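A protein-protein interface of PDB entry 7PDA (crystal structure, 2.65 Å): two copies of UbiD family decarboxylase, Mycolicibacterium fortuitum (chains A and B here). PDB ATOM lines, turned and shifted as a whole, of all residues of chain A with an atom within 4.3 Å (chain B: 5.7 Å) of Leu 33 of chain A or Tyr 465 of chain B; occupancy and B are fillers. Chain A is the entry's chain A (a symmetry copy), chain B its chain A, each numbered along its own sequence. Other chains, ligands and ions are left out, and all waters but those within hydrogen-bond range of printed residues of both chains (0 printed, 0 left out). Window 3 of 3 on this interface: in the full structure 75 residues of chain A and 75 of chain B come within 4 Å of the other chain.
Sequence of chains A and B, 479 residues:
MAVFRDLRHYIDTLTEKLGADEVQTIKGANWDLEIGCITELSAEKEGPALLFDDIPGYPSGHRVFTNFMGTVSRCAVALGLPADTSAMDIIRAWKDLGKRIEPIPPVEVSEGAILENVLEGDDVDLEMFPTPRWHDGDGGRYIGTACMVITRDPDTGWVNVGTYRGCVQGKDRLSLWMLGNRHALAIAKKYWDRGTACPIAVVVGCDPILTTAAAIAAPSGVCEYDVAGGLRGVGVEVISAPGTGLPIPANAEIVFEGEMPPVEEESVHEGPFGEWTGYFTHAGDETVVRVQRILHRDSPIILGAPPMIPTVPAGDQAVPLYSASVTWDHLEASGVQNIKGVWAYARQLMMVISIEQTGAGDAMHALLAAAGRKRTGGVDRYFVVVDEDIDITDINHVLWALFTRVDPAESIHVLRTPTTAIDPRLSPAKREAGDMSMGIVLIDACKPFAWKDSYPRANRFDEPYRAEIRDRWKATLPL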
ATOM      1  N   TRP A  31       0.966  -2.924 -19.928  1.00  0.00           N
ATOM      2  CA  TRP A  31       0.435  -2.573 -18.611  1.00  0.00           C
ATOM      3  C   TRP A  31      -0.342  -1.253 -18.630  1.00  0.00           C
ATOM      4  O   TRP A  31      -1.260  -1.072 -17.832  1.00  0.00           O
ATOM      5  CB  TRP A  31       1.513  -2.563 -17.523  1.00  0.00           C
ATOM      6  CG  TRP A  31       2.601  -1.561 -17.772  1.00  0.00           C
ATOM      7  CD1 TRP A  31       3.808  -1.805 -18.370  1.00  0.00           C
ATOM      8  CD2 TRP A  31       2.582  -0.153 -17.450  1.00  0.00           C
ATOM      9  NE1 TRP A  31       4.543  -0.659 -18.419  1.00  0.00           N
ATOM     10  CE2 TRP A  31       3.824   0.375 -17.867  1.00  0.00           C
ATOM     11  CE3 TRP A  31       1.670   0.702 -16.823  1.00  0.00           C
ATOM     12  CZ2 TRP A  31       4.162   1.718 -17.690  1.00  0.00           C
ATOM     13  CZ3 TRP A  31       1.993   2.033 -16.676  1.00  0.00           C
ATOM     14  CH2 TRP A  31       3.224   2.534 -17.100  1.00  0.00           C
ATOM     15  N   ASP A  32       0.019  -0.327 -19.528  1.00  0.00           N
ATOM     16  CA  ASP A  32      -0.585   0.992 -19.512  1.00  0.00           C
ATOM     17  C   ASP A  32      -1.918   0.936 -20.239  1.00  0.00           C
ATOM     18  O   ASP A  32      -1.926   0.949 -21.461  1.00  0.00           O
ATOM     19  CB  ASP A  32       0.303   2.036 -20.204  1.00  0.00           C
ATOM     20  CG  ASP A  32      -0.063   3.453 -19.801  1.00  0.00           C
ATOM     21  OD1 ASP A  32      -1.259   3.713 -19.512  1.00  0.00           O
ATOM     22  OD2 ASP A  32       0.823   4.271 -19.727  1.00  0.00           O
ATOM     23  N   LEU A  33      -3.028   0.866 -19.491  1.00  0.00           N
ATOM     24  CA  LEU A  33      -4.378   0.996 -20.028  1.00  0.00           C
ATOM     25  C   LEU A  33      -4.805  -0.274 -20.747  1.00  0.00           C
ATOM     26  O   LEU A  33      -5.957  -0.686 -20.627  1.00  0.00           O
ATOM     27  CB  LEU A  33      -4.519   2.201 -20.969  1.00  0.00           C
ATOM     28  CG  LEU A  33      -4.449   3.552 -20.272  1.00  0.00           C
ATOM     29  CD1 LEU A  33      -4.845   4.691 -21.200  1.00  0.00           C
ATOM     30  CD2 LEU A  33      -5.308   3.517 -19.025  1.00  0.00           C
ATOM     31  N   GLU A  34      -3.895  -0.833 -21.546  1.00  0.00           N
ATOM     32  CA  GLU A  34      -4.282  -1.852 -22.495  1.00  0.00           C
ATOM     33  C   GLU A  34      -4.817  -3.112 -21.807  1.00  0.00           C
ATOM     34  O   GLU A  34      -5.880  -3.587 -22.190  1.00  0.00           O
ATOM     35  CB  GLU A  34      -3.146  -2.164 -23.443  1.00  0.00           C
ATOM     36  CG  GLU A  34      -3.608  -3.000 -24.604  1.00  0.00           C
ATOM     37  CD  GLU A  34      -2.507  -3.311 -25.592  1.00  0.00           C
ATOM     38  OE1 GLU A  34      -2.887  -3.641 -26.740  1.00  0.00           O
ATOM     39  OE2 GLU A  34      -1.282  -3.247 -25.210  1.00  0.00           O
ATOM     40  N   ILE A  35      -4.085  -3.651 -20.814  1.00  0.00           N
ATOM     41  CA  ILE A  35      -4.529  -4.781 -19.994  1.00  0.00           C
ATOM     42  C   ILE A  35      -5.896  -4.480 -19.365  1.00  0.00           C
ATOM     43  O   ILE A  35      -6.810  -5.303 -19.404  1.00  0.00           O
ATOM     44  CB  ILE A  35      -3.448  -5.155 -18.955  1.00  0.00           C
ATOM     45  CG1 ILE A  35      -2.222  -5.794 -19.623  1.00  0.00           C
ATOM     46  CG2 ILE A  35      -3.989  -6.044 -17.867  1.00  0.00           C
ATOM     47  CD1 ILE A  35      -1.240  -6.506 -18.682  1.00  0.00           C
ATOM     48  N   GLY A  36      -6.032  -3.295 -18.768  1.00  0.00           N
ATOM     49  CA  GLY A  36      -7.251  -2.962 -18.054  1.00  0.00           C
ATOM     50  C   GLY A  36      -8.445  -2.958 -19.000  1.00  0.00           C
ATOM     51  O   GLY A  36      -9.553  -3.438 -18.675  1.00  0.00           O
ATOM     52  N   CYS A  37      -8.184  -2.450 -20.202  1.00  0.00           N
ATOM     53  CA  CYS A  37      -9.264  -2.187 -21.121  1.00  0.00           C
ATOM     54  C   CYS A  37      -9.759  -3.506 -21.697  1.00  0.00           C
ATOM     55  O   CYS A  37     -10.985  -3.676 -21.872  1.00  0.00           O
ATOM     56  CB  CYS A  37      -8.837  -1.257 -22.236  1.00  0.00           C
ATOM     57  SG  CYS A  37     -10.229  -1.028 -23.360  1.00  0.00           S
ATOM     58  N   ARG A 133      -1.710   0.245 -15.311  1.00  0.00           N
ATOM     59  CA  ARG A 133      -2.532   1.384 -14.947  1.00  0.00           C
ATOM     60  C   ARG A 133      -3.905   1.005 -15.482  1.00  0.00           C
ATOM     61  O   ARG A 133      -4.121   1.025 -16.699  1.00  0.00           O
ATOM     62  CB  ARG A 133      -1.983   2.684 -15.562  1.00  0.00           C
ATOM     63  CG  ARG A 133      -2.914   3.877 -15.392  1.00  0.00           C
ATOM     64  CD  ARG A 133      -2.202   5.198 -15.613  1.00  0.00           C
ATOM     65  NE  ARG A 133      -2.064   5.589 -17.004  1.00  0.00           N
ATOM     66  CZ  ARG A 133      -2.856   6.465 -17.616  1.00  0.00           C
ATOM     67  NH1 ARG A 133      -3.849   7.075 -16.958  1.00  0.00           N
ATOM     68  NH2 ARG A 133      -2.648   6.703 -18.901  1.00  0.00           N
ATOM     69  N   HIS A 135      -7.119   2.068 -15.366  1.00  0.00           N
ATOM     70  CA  HIS A 135      -8.055   2.958 -16.049  1.00  0.00           C
ATOM     71  C   HIS A 135      -7.421   4.334 -16.273  1.00  0.00           C
ATOM     72  O   HIS A 135      -6.649   4.804 -15.443  1.00  0.00           O
ATOM     73  CB  HIS A 135      -9.333   3.113 -15.207  1.00  0.00           C
ATOM     74  CG  HIS A 135     -10.289   1.983 -15.354  1.00  0.00           C
ATOM     75  ND1 HIS A 135     -11.133   1.862 -16.460  1.00  0.00           N
ATOM     76  CD2 HIS A 135     -10.550   0.925 -14.557  1.00  0.00           C
ATOM     77  CE1 HIS A 135     -11.857   0.756 -16.350  1.00  0.00           C
ATOM     78  NE2 HIS A 135     -11.520   0.170 -15.190  1.00  0.00           N
ATOM     79  N   ASP A 136      -7.767   5.000 -17.381  1.00  0.00           N
ATOM     80  CA  ASP A 136      -7.320   6.370 -17.523  1.00  0.00           C
ATOM     81  C   ASP A 136      -7.947   7.162 -16.385  1.00  0.00           C
ATOM     82  O   ASP A 136      -9.136   6.967 -16.112  1.00  0.00           O
ATOM     83  CB  ASP A 136      -7.625   6.945 -18.898  1.00  0.00           C
ATOM     84  CG  ASP A 136      -7.061   8.346 -19.022  1.00  0.00           C
ATOM     85  OD1 ASP A 136      -5.808   8.553 -18.709  1.00  0.00           O
ATOM     86  OD2 ASP A 136      -7.842   9.229 -19.416  1.00  0.00           O
ATOM     87  N   PHE B 461     -13.515   2.813 -19.701  1.00  0.00           N
ATOM     88  CA  PHE B 461     -12.828   3.185 -20.922  1.00  0.00           C
ATOM     89  C   PHE B 461     -13.718   3.930 -21.898  1.00  0.00           C
ATOM     90  O   PHE B 461     -14.869   3.586 -22.155  1.00  0.00           O
ATOM     91  CB  PHE B 461     -12.192   1.981 -21.591  1.00  0.00           C
ATOM     92  CG  PHE B 461     -10.891   1.703 -20.913  1.00  0.00           C
ATOM     93  CD1 PHE B 461      -9.801   2.517 -21.158  1.00  0.00           C
ATOM     94  CD2 PHE B 461     -10.804   0.727 -19.937  1.00  0.00           C
ATOM     95  CE1 PHE B 461      -8.618   2.301 -20.482  1.00  0.00           C
ATOM     96  CE2 PHE B 461      -9.620   0.533 -19.249  1.00  0.00           C
ATOM     97  CZ  PHE B 461      -8.530   1.317 -19.528  1.00  0.00           C
ATOM     98  N   ASP B 462     -13.121   4.987 -22.446  1.00  0.00           N
ATOM     99  CA  ASP B 462     -13.770   5.782 -23.461  1.00  0.00           C
ATOM    100  C   ASP B 462     -14.075   4.889 -24.658  1.00  0.00           C
ATOM    101  O   ASP B 462     -13.448   3.850 -24.807  1.00  0.00           O
ATOM    102  CB  ASP B 462     -12.862   6.947 -23.799  1.00  0.00           C
ATOM    103  CG  ASP B 462     -13.672   8.185 -23.550  1.00  0.00           C
ATOM    104  OD1 ASP B 462     -14.898   8.091 -23.853  1.00  0.00           O
ATOM    105  OD2 ASP B 462     -13.093   9.183 -22.988  1.00  0.00           O
ATOM    106  N   GLU B 463     -15.008   5.321 -25.516  1.00  0.00           N
ATOM    107  CA  GLU B 463     -15.532   4.510 -26.610  1.00  0.00           C
ATOM    108  C   GLU B 463     -14.473   4.305 -27.695  1.00  0.00           C
ATOM    109  O   GLU B 463     -14.277   3.158 -28.103  1.00  0.00           O
ATOM    110  CB  GLU B 463     -16.847   5.109 -27.104  1.00  0.00           C
ATOM    111  CG  GLU B 463     -17.475   4.343 -28.242  1.00  0.00           C
ATOM    112  CD  GLU B 463     -17.396   2.858 -27.965  1.00  0.00           C
ATOM    113  OE1 GLU B 463     -16.809   2.164 -28.800  1.00  0.00           O
ATOM    114  OE2 GLU B 463     -17.918   2.405 -26.905  1.00  0.00           O
ATOM    115  N   PRO B 464     -13.772   5.372 -28.179  1.00  0.00           N
ATOM    116  CA  PRO B 464     -12.673   5.250 -29.144  1.00  0.00           C
ATOM    117  C   PRO B 464     -11.631   4.184 -28.800  1.00  0.00           C
ATOM    118  O   PRO B 464     -11.341   3.316 -29.609  1.00  0.00           O
ATOM    119  CB  PRO B 464     -11.940   6.612 -29.084  1.00  0.00           C
ATOM    120  CG  PRO B 464     -12.573   7.375 -27.921  1.00  0.00           C
ATOM    121  CD  PRO B 464     -13.960   6.781 -27.793  1.00  0.00           C
ATOM    122  N   TYR B 465     -11.075   4.263 -27.592  1.00  0.00           N
ATOM    123  CA  TYR B 465     -10.163   3.277 -27.041  1.00  0.00           C
ATOM    124  C   TYR B 465     -10.823   1.890 -26.985  1.00  0.00           C
ATOM    125  O   TYR B 465     -10.320   0.913 -27.535  1.00  0.00           O
ATOM    126  CB  TYR B 465      -9.587   3.830 -25.728  1.00  0.00           C
ATOM    127  CG  TYR B 465      -8.355   3.089 -25.307  1.00  0.00           C
ATOM    128  CD1 TYR B 465      -7.095   3.492 -25.719  1.00  0.00           C
ATOM    129  CD2 TYR B 465      -8.452   1.924 -24.575  1.00  0.00           C
ATOM    130  CE1 TYR B 465      -5.954   2.786 -25.374  1.00  0.00           C
ATOM    131  CE2 TYR B 465      -7.328   1.200 -24.232  1.00  0.00           C
ATOM    132  CZ  TYR B 465      -6.076   1.634 -24.620  1.00  0.00           C
ATOM    133  OH  TYR B 465      -4.984   0.895 -24.263  1.00  0.00           O
ATOM    134  N   ARG B 466     -11.987   1.782 -26.354  1.00  0.00           N
ATOM    135  CA  ARG B 466     -12.734   0.535 -26.366  1.00  0.00           C
ATOM    136  C   ARG B 466     -12.700  -0.066 -27.776  1.00  0.00           C
ATOM    137  O   ARG B 466     -12.481  -1.274 -27.970  1.00  0.00           O
ATOM    138  CB  ARG B 466     -14.123   0.721 -25.747  1.00  0.00           C
ATOM    139  CG  ARG B 466     -14.093   0.871 -24.230  1.00  0.00           C
ATOM    140  CD  ARG B 466     -15.371   1.189 -23.488  1.00  0.00           C
ATOM    141  NE  ARG B 466     -16.329   0.126 -23.735  1.00  0.00           N
ATOM    142  CZ  ARG B 466     -16.846  -0.735 -22.842  1.00  0.00           C
ATOM    143  NH1 ARG B 466     -16.553  -0.673 -21.545  1.00  0.00           N
ATOM    144  NH2 ARG B 466     -17.690  -1.653 -23.285  1.00  0.00           N
ATOM    145  N   ALA B 467     -12.836   0.802 -28.783  1.00  0.00           N
ATOM    146  CA  ALA B 467     -12.842   0.319 -30.158  1.00  0.00           C
ATOM    147  C   ALA B 467     -11.422   0.137 -30.692  1.00  0.00           C
ATOM    148  O   ALA B 467     -11.200  -0.695 -31.553  1.00  0.00           O
ATOM    149  CB  ALA B 467     -13.722   1.165 -31.050  1.00  0.00           C
ATOM    150  N   GLU B 468     -10.430   0.826 -30.139  1.00  0.00           N
ATOM    151  CA  GLU B 468      -9.062   0.551 -30.574  1.00  0.00           C
ATOM    152  C   GLU B 468      -8.636  -0.854 -30.130  1.00  0.00           C
ATOM    153  O   GLU B 468      -8.173  -1.679 -30.924  1.00  0.00           O
ATOM    154  CB  GLU B 468      -8.103   1.651 -30.129  1.00  0.00           C
ATOM    155  CG  GLU B 468      -6.710   1.463 -30.683  1.00  0.00           C
ATOM    156  CD  GLU B 468      -5.663   2.405 -30.116  1.00  0.00           C
ATOM    157  OE1 GLU B 468      -6.033   3.483 -29.613  1.00  0.00           O
ATOM    158  OE2 GLU B 468      -4.465   2.048 -30.154  1.00  0.00           O
ATOM    159  N   ILE B 469      -8.858  -1.147 -28.851  1.00  0.00           N
ATOM    160  CA  ILE B 469      -8.510  -2.453 -28.322  1.00  0.00           C
ATOM    161  C   ILE B 469      -9.363  -3.548 -28.977  1.00  0.00           C
ATOM    162  O   ILE B 469      -8.856  -4.618 -29.280  1.00  0.00           O
ATOM    163  CB  ILE B 469      -8.598  -2.427 -26.783  1.00  0.00           C
ATOM    164  CG1 ILE B 469      -7.726  -1.324 -26.166  1.00  0.00           C
ATOM    165  CG2 ILE B 469      -8.264  -3.785 -26.205  1.00  0.00           C
ATOM    166  CD1 ILE B 469      -6.256  -1.274 -26.630  1.00  0.00           C
ATOM    167  N   ARG B 470     -10.649  -3.290 -29.214  1.00  0.00           N
ATOM    168  CA  ARG B 470     -11.530  -4.314 -29.779  1.00  0.00           C
ATOM    169  C   ARG B 470     -11.016  -4.779 -31.156  1.00  0.00           C
ATOM    170  O   ARG B 470     -10.792  -5.967 -31.410  1.00  0.00           O
ATOM    171  CB  ARG B 470     -12.973  -3.787 -29.801  1.00  0.00           C
ATOM    172  CG  ARG B 470     -14.050  -4.830 -30.061  1.00  0.00           C
ATOM    173  CD  ARG B 470     -15.462  -4.251 -29.940  1.00  0.00           C
ATOM    174  NE  ARG B 470     -15.655  -3.116 -29.013  1.00  0.00           N
ATOM    175  CZ  ARG B 470     -15.947  -3.190 -27.700  1.00  0.00           C
ATOM    176  NH1 ARG B 470     -16.051  -4.365 -27.088  1.00  0.00           N
ATOM    177  NH2 ARG B 470     -16.108  -2.076 -26.998  1.00  0.00           N
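OH of Tyr 465 of chain B sits close to N of Glu 34 of chain A (3.4 Å).
The backbone NH (N) of Leu 33 of chain A is in hydrogen-bond range of the backbone carbonyl oxygen (O) of Arg 133 of chain A (3.0 Å).
Leu 33 of chain A touches Phe 461 of chain B (O to CZ, 3.4 Å).
CB of Leu 33 of chain A touches OH of Tyr 465 of chain B, 3.6 Å away.
Ile 469 of chain B touches Glu 34 of chain A.
Phe 461 of chain B touches Gly 36 of chain A (CE2 to C, 3.7 Å).
Phe 461 of chain B touches Cys 37 of chain A.
Cys 37 of chain A touches Tyr 465 of chain B (CB to CE2, 3.5 Å).
Cys 37 of chain A touches Ile 469 of chain B.
His 135 of chain A touches Phe 461 of chain B.
Of chain B, only Phe 461 (3.4 Å) and Tyr 465 (3.6 Å) come within 4 Å of Leu 33 of chain A.
Printed residues of chain A within 4 Å of Tyr 465 of chain B: Leu 33, Glu 34 and Cys 37.
Of the printed residues of chain A, Phe 461 of chain B touches Leu 33, Gly 36, Cys 37 and His 135.
Of the printed residues of chain B, Cys 37 of chain A touches Phe 461 (3.3 Å), Tyr 465 (3.5 Å) and Ile 469 (3.8 Å).
Of the printed residues of chain B, His 135 of chain A touches Phe 461.
Printed residues of chain B within 4 Å of Gly 36 of chain A: Phe 461 (3.7 Å).
Pro 464 of chain B touches none of the printed residues of chain A.
Asp 136 of chain A touches none of the printed residues of chain B.
The nearest printed residue of chain B that does not touch Leu 33 of chain A is Ile 469 of chain B (5.8 Å).
The nearest residue of chain A that does not touch Tyr 465 of chain B is Asp 32 of chain A (4.1 Å).
The nearest printed residue of chain B that does not touch His 135 of chain A is Asp 462 of chain B (7.0 Å).
Of the 10 printed residues of chain B, 3 touch a printed residue of chain A.
Hydrophobic or aromatic side chains of chain B that line the printed part of chain A: Phe 461, Tyr 465 and Ile 469.
Hydrophobic or aromatic side chains of chain A that line the printed part of chain B: Leu 33 and His 135.
Among the printed residues, no Asp or Glu carboxylate lies within 4 Å of a Lys or Arg side-chain nitrogen of the other chain.
No position is printed for both chains.
Of the 9 pairs that touch across the chains among the printed residues, none has its exchanged pair printed and touching as well.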
